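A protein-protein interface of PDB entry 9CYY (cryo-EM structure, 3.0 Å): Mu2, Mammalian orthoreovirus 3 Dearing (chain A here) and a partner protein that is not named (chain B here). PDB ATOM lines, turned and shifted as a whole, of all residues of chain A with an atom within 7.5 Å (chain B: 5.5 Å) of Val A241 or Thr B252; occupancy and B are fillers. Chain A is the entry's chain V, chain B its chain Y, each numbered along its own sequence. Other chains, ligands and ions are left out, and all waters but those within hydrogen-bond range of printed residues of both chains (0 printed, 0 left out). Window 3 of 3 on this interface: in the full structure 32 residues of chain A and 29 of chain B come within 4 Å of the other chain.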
ATOM      1  N   GLY A  57       6.676   2.270  16.873  1.00  0.00           N
ATOM      2  CA  GLY A  57       6.199   1.020  17.446  1.00  0.00           C
ATOM      3  C   GLY A  57       7.307   0.020  17.709  1.00  0.00           C
ATOM      4  O   GLY A  57       7.386  -0.567  18.791  1.00  0.00           O
ATOM      5  N   ILE A  60       9.658   1.154  20.529  1.00  0.00           N
ATOM      6  CA  ILE A  60       9.032   0.964  21.834  1.00  0.00           C
ATOM      7  C   ILE A  60       9.031  -0.511  22.217  1.00  0.00           C
ATOM      8  O   ILE A  60       9.370  -0.875  23.351  1.00  0.00           O
ATOM      9  CB  ILE A  60       7.608   1.550  21.836  1.00  0.00           C
ATOM     10  CG1 ILE A  60       7.660   3.077  21.803  1.00  0.00           C
ATOM     11  CG2 ILE A  60       6.833   1.065  23.051  1.00  0.00           C
ATOM     12  CD1 ILE A  60       6.327   3.740  22.063  1.00  0.00           C
ATOM     13  N   ASP A  61       8.665  -1.382  21.274  1.00  0.00           N
ATOM     14  CA  ASP A  61       8.608  -2.811  21.560  1.00  0.00           C
ATOM     15  C   ASP A  61       9.981  -3.345  21.947  1.00  0.00           C
ATOM     16  O   ASP A  61      10.106  -4.160  22.868  1.00  0.00           O
ATOM     17  CB  ASP A  61       8.057  -3.561  20.349  1.00  0.00           C
ATOM     18  CG  ASP A  61       6.591  -3.269  20.101  1.00  0.00           C
ATOM     19  OD1 ASP A  61       5.870  -2.977  21.077  1.00  0.00           O
ATOM     20  OD2 ASP A  61       6.161  -3.329  18.930  1.00  0.00           O
ATOM     21  N   VAL A  64      10.968  -2.219  25.447  1.00  0.00           N
ATOM     22  CA  VAL A  64      10.247  -2.915  26.510  1.00  0.00           C
ATOM     23  C   VAL A  64      11.088  -4.022  27.134  1.00  0.00           C
ATOM     24  O   VAL A  64      11.035  -4.228  28.352  1.00  0.00           O
ATOM     25  CB  VAL A  64       8.911  -3.482  25.983  1.00  0.00           C
ATOM     26  CG1 VAL A  64       8.241  -4.335  27.040  1.00  0.00           C
ATOM     27  CG2 VAL A  64       7.983  -2.362  25.593  1.00  0.00           C
ATOM     28  N   TYR A 235       3.576   4.334  27.393  1.00  0.00           N
ATOM     29  CA  TYR A 235       2.630   3.609  28.232  1.00  0.00           C
ATOM     30  C   TYR A 235       1.457   3.084  27.420  1.00  0.00           C
ATOM     31  O   TYR A 235       1.001   1.956  27.641  1.00  0.00           O
ATOM     32  CB  TYR A 235       2.148   4.502  29.372  1.00  0.00           C
ATOM     33  CG  TYR A 235       3.018   4.413  30.600  1.00  0.00           C
ATOM     34  CD1 TYR A 235       4.345   4.816  30.569  1.00  0.00           C
ATOM     35  CD2 TYR A 235       2.517   3.903  31.787  1.00  0.00           C
ATOM     36  CE1 TYR A 235       5.142   4.727  31.690  1.00  0.00           C
ATOM     37  CE2 TYR A 235       3.306   3.809  32.912  1.00  0.00           C
ATOM     38  CZ  TYR A 235       4.616   4.222  32.859  1.00  0.00           C
ATOM     39  OH  TYR A 235       5.402   4.127  33.981  1.00  0.00           O
ATOM     40  N   GLN A 236       0.954   3.878  26.471  1.00  0.00           N
ATOM     41  CA  GLN A 236      -0.141   3.414  25.627  1.00  0.00           C
ATOM     42  C   GLN A 236       0.249   2.164  24.856  1.00  0.00           C
ATOM     43  O   GLN A 236      -0.487   1.172  24.850  1.00  0.00           O
ATOM     44  CB  GLN A 236      -0.573   4.510  24.656  1.00  0.00           C
ATOM     45  CG  GLN A 236      -1.765   4.096  23.815  1.00  0.00           C
ATOM     46  CD  GLN A 236      -2.246   5.183  22.883  1.00  0.00           C
ATOM     47  OE1 GLN A 236      -1.670   6.269  22.821  1.00  0.00           O
ATOM     48  NE2 GLN A 236      -3.295   4.884  22.126  1.00  0.00           N
ATOM     49  N   ARG A 237       1.406   2.196  24.192  1.00  0.00           N
ATOM     50  CA  ARG A 237       1.817   1.047  23.393  1.00  0.00           C
ATOM     51  C   ARG A 237       2.032  -0.182  24.266  1.00  0.00           C
ATOM     52  O   ARG A 237       1.586  -1.287  23.923  1.00  0.00           O
ATOM     53  CB  ARG A 237       3.085   1.384  22.609  1.00  0.00           C
ATOM     54  CG  ARG A 237       3.529   0.305  21.637  1.00  0.00           C
ATOM     55  CD  ARG A 237       2.575   0.192  20.461  1.00  0.00           C
ATOM     56  NE  ARG A 237       3.056  -0.754  19.461  1.00  0.00           N
ATOM     57  CZ  ARG A 237       2.354  -1.154  18.410  1.00  0.00           C
ATOM     58  NH1 ARG A 237       1.126  -0.713  18.190  1.00  0.00           N
ATOM     59  NH2 ARG A 237       2.897  -2.016  17.557  1.00  0.00           N
ATOM     60  N   VAL A 238       2.699  -0.007  25.411  1.00  0.00           N
ATOM     61  CA  VAL A 238       2.970  -1.142  26.289  1.00  0.00           C
ATOM     62  C   VAL A 238       1.667  -1.754  26.786  1.00  0.00           C
ATOM     63  O   VAL A 238       1.483  -2.976  26.755  1.00  0.00           O
ATOM     64  CB  VAL A 238       3.873  -0.713  27.458  1.00  0.00           C
ATOM     65  CG1 VAL A 238       3.906  -1.794  28.525  1.00  0.00           C
ATOM     66  CG2 VAL A 238       5.269  -0.413  26.958  1.00  0.00           C
ATOM     67  N   LYS A 239       0.736  -0.912  27.242  1.00  0.00           N
ATOM     68  CA  LYS A 239      -0.514  -1.431  27.781  1.00  0.00           C
ATOM     69  C   LYS A 239      -1.363  -2.062  26.686  1.00  0.00           C
ATOM     70  O   LYS A 239      -2.087  -3.032  26.934  1.00  0.00           O
ATOM     71  CB  LYS A 239      -1.275  -0.312  28.497  1.00  0.00           C
ATOM     72  CG  LYS A 239      -2.592  -0.732  29.144  1.00  0.00           C
ATOM     73  CD  LYS A 239      -3.784  -0.494  28.230  1.00  0.00           C
ATOM     74  CE  LYS A 239      -4.064   0.990  28.072  1.00  0.00           C
ATOM     75  NZ  LYS A 239      -5.235   1.241  27.191  1.00  0.00           N
ATOM     76  N   SER A 240      -1.289  -1.531  25.465  1.00  0.00           N
ATOM     77  CA  SER A 240      -2.082  -2.080  24.377  1.00  0.00           C
ATOM     78  C   SER A 240      -1.534  -3.396  23.846  1.00  0.00           C
ATOM     79  O   SER A 240      -2.312  -4.190  23.309  1.00  0.00           O
ATOM     80  CB  SER A 240      -2.183  -1.068  23.235  1.00  0.00           C
ATOM     81  OG  SER A 240      -0.918  -0.842  22.639  1.00  0.00           O
ATOM     82  N   VAL A 241      -0.229  -3.651  23.971  1.00  0.00           N
ATOM     83  CA  VAL A 241       0.379  -4.867  23.445  1.00  0.00           C
ATOM     84  C   VAL A 241       0.473  -5.961  24.506  1.00  0.00           C
ATOM     85  O   VAL A 241       0.054  -7.100  24.276  1.00  0.00           O
ATOM     86  CB  VAL A 241       1.765  -4.585  22.829  1.00  0.00           C
ATOM     87  CG1 VAL A 241       2.416  -5.883  22.386  1.00  0.00           C
ATOM     88  CG2 VAL A 241       1.633  -3.631  21.654  1.00  0.00           C
ATOM     89  N   HIS A 242       1.020  -5.636  25.676  1.00  0.00           N
ATOM     90  CA  HIS A 242       1.309  -6.620  26.718  1.00  0.00           C
ATOM     91  C   HIS A 242       0.393  -6.469  27.930  1.00  0.00           C
ATOM     92  O   HIS A 242       0.844  -6.540  29.075  1.00  0.00           O
ATOM     93  CB  HIS A 242       2.768  -6.537  27.157  1.00  0.00           C
ATOM     94  CG  HIS A 242       3.747  -6.608  26.028  1.00  0.00           C
ATOM     95  ND1 HIS A 242       4.280  -5.485  25.434  1.00  0.00           N
ATOM     96  CD2 HIS A 242       4.295  -7.668  25.390  1.00  0.00           C
ATOM     97  CE1 HIS A 242       5.115  -5.850  24.477  1.00  0.00           C
ATOM     98  NE2 HIS A 242       5.140  -7.170  24.428  1.00  0.00           N
ATOM     99  N   ALA A 243      -0.903  -6.258  27.692  1.00  0.00           N
ATOM    100  CA  ALA A 243      -1.827  -5.980  28.790  1.00  0.00           C
ATOM    101  C   ALA A 243      -1.888  -7.128  29.792  1.00  0.00           C
ATOM    102  O   ALA A 243      -1.928  -6.899  31.006  1.00  0.00           O
ATOM    103  CB  ALA A 243      -3.221  -5.687  28.238  1.00  0.00           C
ATOM    104  N   ASN A 244      -1.897  -8.370  29.308  1.00  0.00           N
ATOM    105  CA  ASN A 244      -2.162  -9.511  30.177  1.00  0.00           C
ATOM    106  C   ASN A 244      -0.960  -9.942  31.007  1.00  0.00           C
ATOM    107  O   ASN A 244      -1.122 -10.788  31.893  1.00  0.00           O
ATOM    108  CB  ASN A 244      -2.656 -10.696  29.345  1.00  0.00           C
ATOM    109  CG  ASN A 244      -4.088 -10.528  28.882  1.00  0.00           C
ATOM    110  OD1 ASN A 244      -4.980 -10.243  29.679  1.00  0.00           O
ATOM    111  ND2 ASN A 244      -4.315 -10.701  27.587  1.00  0.00           N
ATOM    112  N   ILE A 245       0.230  -9.399  30.756  1.00  0.00           N
ATOM    113  CA  ILE A 245       1.432  -9.875  31.436  1.00  0.00           C
ATOM    114  C   ILE A 245       2.128  -8.747  32.187  1.00  0.00           C
ATOM    115  O   ILE A 245       3.355  -8.754  32.332  1.00  0.00           O
ATOM    116  CB  ILE A 245       2.399 -10.539  30.439  1.00  0.00           C
ATOM    117  CG1 ILE A 245       2.707  -9.590  29.282  1.00  0.00           C
ATOM    118  CG2 ILE A 245       1.822 -11.848  29.927  1.00  0.00           C
ATOM    119  CD1 ILE A 245       3.786 -10.090  28.355  1.00  0.00           C
ATOM    120  N   LEU A 246       1.359  -7.779  32.678  1.00  0.00           N
ATOM    121  CA  LEU A 246       1.898  -6.664  33.446  1.00  0.00           C
ATOM    122  C   LEU A 246       1.404  -6.743  34.884  1.00  0.00           C
ATOM    123  O   LEU A 246       0.227  -7.029  35.126  1.00  0.00           O
ATOM    124  CB  LEU A 246       1.503  -5.322  32.828  1.00  0.00           C
ATOM    125  CG  LEU A 246       2.219  -4.929  31.535  1.00  0.00           C
ATOM    126  CD1 LEU A 246       1.479  -3.802  30.838  1.00  0.00           C
ATOM    127  CD2 LEU A 246       3.659  -4.537  31.815  1.00  0.00           C
ATOM    128  N   HIS B 249      -3.064  -3.037  13.439  1.00  0.00           N
ATOM    129  CA  HIS B 249      -2.825  -3.313  14.846  1.00  0.00           C
ATOM    130  C   HIS B 249      -4.116  -3.099  15.620  1.00  0.00           C
ATOM    131  O   HIS B 249      -4.817  -2.105  15.419  1.00  0.00           O
ATOM    132  CB  HIS B 249      -1.714  -2.421  15.407  1.00  0.00           C
ATOM    133  CG  HIS B 249      -1.317  -2.762  16.808  1.00  0.00           C
ATOM    134  ND1 HIS B 249      -1.959  -2.242  17.910  1.00  0.00           N
ATOM    135  CD2 HIS B 249      -0.342  -3.570  17.288  1.00  0.00           C
ATOM    136  CE1 HIS B 249      -1.399  -2.715  19.009  1.00  0.00           C
ATOM    137  NE2 HIS B 249      -0.415  -3.523  18.658  1.00  0.00           N
ATOM    138  N   ALA B 250      -4.418  -4.032  16.518  1.00  0.00           N
ATOM    139  CA  ALA B 250      -5.657  -3.985  17.276  1.00  0.00           C
ATOM    140  C   ALA B 250      -5.356  -4.103  18.762  1.00  0.00           C
ATOM    141  O   ALA B 250      -4.372  -4.728  19.165  1.00  0.00           O
ATOM    142  CB  ALA B 250      -6.624  -5.096  16.848  1.00  0.00           C
ATOM    143  N   ASP B 251      -6.215  -3.489  19.571  1.00  0.00           N
ATOM    144  CA  ASP B 251      -6.064  -3.560  21.017  1.00  0.00           C
ATOM    145  C   ASP B 251      -6.312  -4.979  21.507  1.00  0.00           C
ATOM    146  O   ASP B 251      -7.151  -5.704  20.965  1.00  0.00           O
ATOM    147  CB  ASP B 251      -7.031  -2.595  21.700  1.00  0.00           C
ATOM    148  CG  ASP B 251      -6.598  -1.152  21.576  1.00  0.00           C
ATOM    149  OD1 ASP B 251      -5.885  -0.826  20.604  1.00  0.00           O
ATOM    150  OD2 ASP B 251      -6.972  -0.342  22.450  1.00  0.00           O
ATOM    151  N   THR B 252      -5.577  -5.374  22.537  1.00  0.00           N
ATOM    152  CA  THR B 252      -5.732  -6.717  23.079  1.00  0.00           C
ATOM    153  C   THR B 252      -6.585  -6.676  24.334  1.00  0.00           C
ATOM    154  O   THR B 252      -6.302  -5.883  25.242  1.00  0.00           O
ATOM    155  CB  THR B 252      -4.375  -7.326  23.402  1.00  0.00           C
ATOM    156  OG1 THR B 252      -3.906  -6.808  24.651  1.00  0.00           O
ATOM    157  CG2 THR B 252      -3.383  -6.969  22.320  1.00  0.00           C
ATOM    158  N   PRO B 253      -7.622  -7.502  24.421  1.00  0.00           N
ATOM    159  CA  PRO B 253      -8.459  -7.510  25.621  1.00  0.00           C
ATOM    160  C   PRO B 253      -7.694  -8.007  26.835  1.00  0.00           C
ATOM    161  O   PRO B 253      -6.752  -8.795  26.729  1.00  0.00           O
ATOM    162  CB  PRO B 253      -9.594  -8.468  25.251  1.00  0.00           C
ATOM    163  CG  PRO B 253      -8.988  -9.369  24.232  1.00  0.00           C
ATOM    164  CD  PRO B 253      -8.047  -8.516  23.443  1.00  0.00           C
ATOM    165  N   ARG B 254      -8.114  -7.530  28.003  1.00  0.00           N
ATOM    166  CA  ARG B 254      -7.490  -7.901  29.271  1.00  0.00           C
ATOM    167  C   ARG B 254      -8.294  -9.048  29.872  1.00  0.00           C
ATOM    168  O   ARG B 254      -9.397  -8.847  30.382  1.00  0.00           O
ATOM    169  CB  ARG B 254      -7.435  -6.702  30.208  1.00  0.00           C
ATOM    170  CG  ARG B 254      -6.815  -6.994  31.558  1.00  0.00           C
ATOM    171  CD  ARG B 254      -5.337  -7.308  31.416  1.00  0.00           C
ATOM    172  NE  ARG B 254      -4.717  -7.600  32.702  1.00  0.00           N
ATOM    173  CZ  ARG B 254      -4.172  -6.687  33.493  1.00  0.00           C
ATOM    174  NH1 ARG B 254      -4.150  -5.408  33.159  1.00  0.00           N
ATOM    175  NH2 ARG B 254      -3.636  -7.068  34.649  1.00  0.00           N
ATOM    176  N   THR B 912       5.008 -11.280  19.747  1.00  0.00           N
ATOM    177  CA  THR B 912       3.857 -11.996  20.287  1.00  0.00           C
ATOM    178  C   THR B 912       2.525 -11.423  19.808  1.00  0.00           C
ATOM    179  O   THR B 912       1.475 -11.733  20.396  1.00  0.00           O
ATOM    180  CB  THR B 912       3.894 -11.992  21.819  1.00  0.00           C
ATOM    181  OG1 THR B 912       3.462 -10.715  22.303  1.00  0.00           O
ATOM    182  CG2 THR B 912       5.302 -12.270  22.327  1.00  0.00           C
ATOM    183  N   GLU B 913       2.538 -10.602  18.756  1.00  0.00           N
ATOM    184  CA  GLU B 913       1.305  -9.972  18.303  1.00  0.00           C
ATOM    185  C   GLU B 913       0.291 -10.999  17.820  1.00  0.00           C
ATOM    186  O   GLU B 913      -0.915 -10.796  17.984  1.00  0.00           O
ATOM    187  CB  GLU B 913       1.606  -8.956  17.204  1.00  0.00           C
ATOM    188  CG  GLU B 913       2.394  -7.752  17.689  1.00  0.00           C
ATOM    189  CD  GLU B 913       2.061  -6.488  16.923  1.00  0.00           C
ATOM    190  OE1 GLU B 913       0.963  -6.421  16.332  1.00  0.00           O
ATOM    191  OE2 GLU B 913       2.897  -5.560  16.912  1.00  0.00           O
ATOM    192  N   SER B 916      -1.463 -12.262  20.772  1.00  0.00           N
ATOM    193  CA  SER B 916      -2.485 -11.300  21.181  1.00  0.00           C
ATOM    194  C   SER B 916      -3.719 -11.367  20.279  1.00  0.00           C
ATOM    195  O   SER B 916      -4.862 -11.275  20.755  1.00  0.00           O
ATOM    196  CB  SER B 916      -1.893  -9.895  21.178  1.00  0.00           C
ATOM    197  OG  SER B 916      -1.801  -9.390  19.858  1.00  0.00           O
ATOM    198  N   GLN B 919      -6.368 -13.993  21.204  1.00  0.00           N
ATOM    199  CA  GLN B 919      -7.272 -13.575  22.270  1.00  0.00           C
ATOM    200  C   GLN B 919      -8.291 -12.568  21.759  1.00  0.00           C
ATOM    201  O   GLN B 919      -9.471 -12.608  22.141  1.00  0.00           O
ATOM    202  CB  GLN B 919      -6.468 -12.984  23.425  1.00  0.00           C
ATOM    203  CG  GLN B 919      -5.270 -13.821  23.827  1.00  0.00           C
ATOM    204  CD  GLN B 919      -4.610 -13.323  25.094  1.00  0.00           C
ATOM    205  OE1 GLN B 919      -4.702 -12.144  25.431  1.00  0.00           O
ATOM    206  NE2 GLN B 919      -3.937 -14.218  25.803  1.00  0.00           N
ATOM    207  N   ARG B 920      -7.851 -11.651  20.895  1.00  0.00           N
ATOM    208  CA  ARG B 920      -8.781 -10.673  20.334  1.00  0.00           C
ATOM    209  C   ARG B 920      -9.900 -11.360  19.554  1.00  0.00           C
ATOM    210  O   ARG B 920     -11.076 -10.994  19.683  1.00  0.00           O
ATOM    211  CB  ARG B 920      -8.028  -9.688  19.442  1.00  0.00           C
ATOM    212  CG  ARG B 920      -8.924  -8.682  18.754  1.00  0.00           C
ATOM    213  CD  ARG B 920      -9.706  -7.876  19.772  1.00  0.00           C
ATOM    214  NE  ARG B 920      -9.719  -6.455  19.450  1.00  0.00           N
ATOM    215  CZ  ARG B 920     -10.698  -5.847  18.797  1.00  0.00           C
ATOM    216  NH1 ARG B 920     -11.765  -6.508  18.379  1.00  0.00           N
ATOM    217  NH2 ARG B 920     -10.607  -4.543  18.557  1.00  0.00           N
ATOM    218  N   PHE B 977     -13.955  -4.863  28.988  1.00  0.00           N
ATOM    219  CA  PHE B 977     -12.716  -5.484  28.536  1.00  0.00           C
ATOM    220  C   PHE B 977     -11.647  -4.479  28.127  1.00  0.00           C
ATOM    221  O   PHE B 977     -10.609  -4.886  27.596  1.00  0.00           O
ATOM    222  CB  PHE B 977     -12.996  -6.450  27.386  1.00  0.00           C
ATOM    223  CG  PHE B 977     -13.506  -7.781  27.837  1.00  0.00           C
ATOM    224  CD1 PHE B 977     -12.648  -8.704  28.404  1.00  0.00           C
ATOM    225  CD2 PHE B 977     -14.844  -8.107  27.713  1.00  0.00           C
ATOM    226  CE1 PHE B 977     -13.109  -9.928  28.829  1.00  0.00           C
ATOM    227  CE2 PHE B 977     -15.311  -9.330  28.136  1.00  0.00           C
ATOM    228  CZ  PHE B 977     -14.441 -10.242  28.696  1.00  0.00           C
ATOM    229  N   ASP B 978     -11.871  -3.189  28.364  1.00  0.00           N
ATOM    230  CA  ASP B 978     -10.852  -2.157  28.169  1.00  0.00           C
ATOM    231  C   ASP B 978     -10.373  -2.132  26.718  1.00  0.00           C
ATOM    232  O   ASP B 978      -9.208  -2.385  26.406  1.00  0.00           O
ATOM    233  CB  ASP B 978      -9.685  -2.366  29.140  1.00  0.00           C
ATOM    234  CG  ASP B 978      -8.697  -1.211  29.134  1.00  0.00           C
ATOM    235  OD1 ASP B 978      -8.887  -0.252  28.357  1.00  0.00           O
ATOM    236  OD2 ASP B 978      -7.722  -1.266  29.911  1.00  0.00           O
ATOM    237  N   LEU B 979     -11.308  -1.823  25.826  1.00  0.00           N
ATOM    238  CA  LEU B 979     -11.036  -1.701  24.401  1.00  0.00           C
ATOM    239  C   LEU B 979     -11.481  -0.326  23.933  1.00  0.00           C
ATOM    240  O   LEU B 979     -12.538   0.160  24.348  1.00  0.00           O
ATOM    241  CB  LEU B 979     -11.754  -2.795  23.609  1.00  0.00           C
ATOM    242  CG  LEU B 979     -11.231  -4.216  23.805  1.00  0.00           C
ATOM    243  CD1 LEU B 979     -12.293  -5.227  23.425  1.00  0.00           C
ATOM    244  CD2 LEU B 979      -9.971  -4.434  22.991  1.00  0.00           C
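Val A241 touches just these residues of chain B: His B249 (3.6 Å) and Thr B252 (3.96 Å). Of chain A, only Ser A240, Val A241 and Ala A243 come within 4 Å of Thr B252. Of the printed residues of chain A, Pro B253 touches Asn A244. Printed residues of chain B within 4 Å of Arg A237: His B249 and Glu B913. Printed residues of chain A within 4 Å of Gln B919: Asn A244 (2.6 Å). Of the printed residues of chain A, Glu B913 touches Arg A237. Of the printed residues of chain B, Ser A240 touches Thr B252. The nearest residue of chain A that does not touch Thr B252 is Lys A239 (4.8 Å). The nearest printed residue of chain B that does not touch Leu A246 is Thr B252 (8.7 Å).
Of the 16 printed residues of chain A, 6 touch a printed residue of chain B. Of the 14 printed residues of chain B, 6 touch a printed residue of chain A. Hydrophobic or aromatic side chains of chain B within 4 Å of the printed part of chain A: His B249.
Among the printed residues, pairs that only touch across the chains: Asn A244 with Arg B254 (3.4 Å), Val A241 with His B249 (3.6 Å), Ala A243 with Thr B252 (3.8 Å), Leu A246 with Arg B254 (3.9 Å) and Val A241 with Thr B252 (3.96 Å).
The backbone carbonyl oxygen (O) of Pro B253 is in hydrogen-bond range of the side-chain amide nitrogen (ND2) of Asn A244, 3.2 Å away. NE of Arg B254 sits at hydrogen-bond distance from O of Ala A243 (3.3 Å). The backbone carbonyl oxygen (O) of Ser A240 lies close to the side-chain hydroxyl (OG1) of Thr B252 (3.3 Å). NH2 of Arg A237 is in salt-bridge range of OE2 of Glu B913. NE2 of His B249 sits at hydrogen-bond distance from NH1 of Arg A237 (3.2 Å). The side-chain amide oxygen (OE1) of Gln B919 sits at hydrogen-bond distance from the side-chain amide nitrogen (ND2) of Asn A244 (2.6 Å).
O of Glu B913 is in hydrogen-bond range of OG of Ser B916, at 2.5 Å. OD2 of Asp A61 is in salt-bridge range of NH2 of Arg A237. The side-chain hydroxyl (OG) of Ser A240 is in hydrogen-bond range of the backbone carbonyl oxygen (O) of Gln A236 (3.0 Å). O of Arg A237 lies within hydrogen-bond range of OG of Ser A240, 2.8 Å away.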
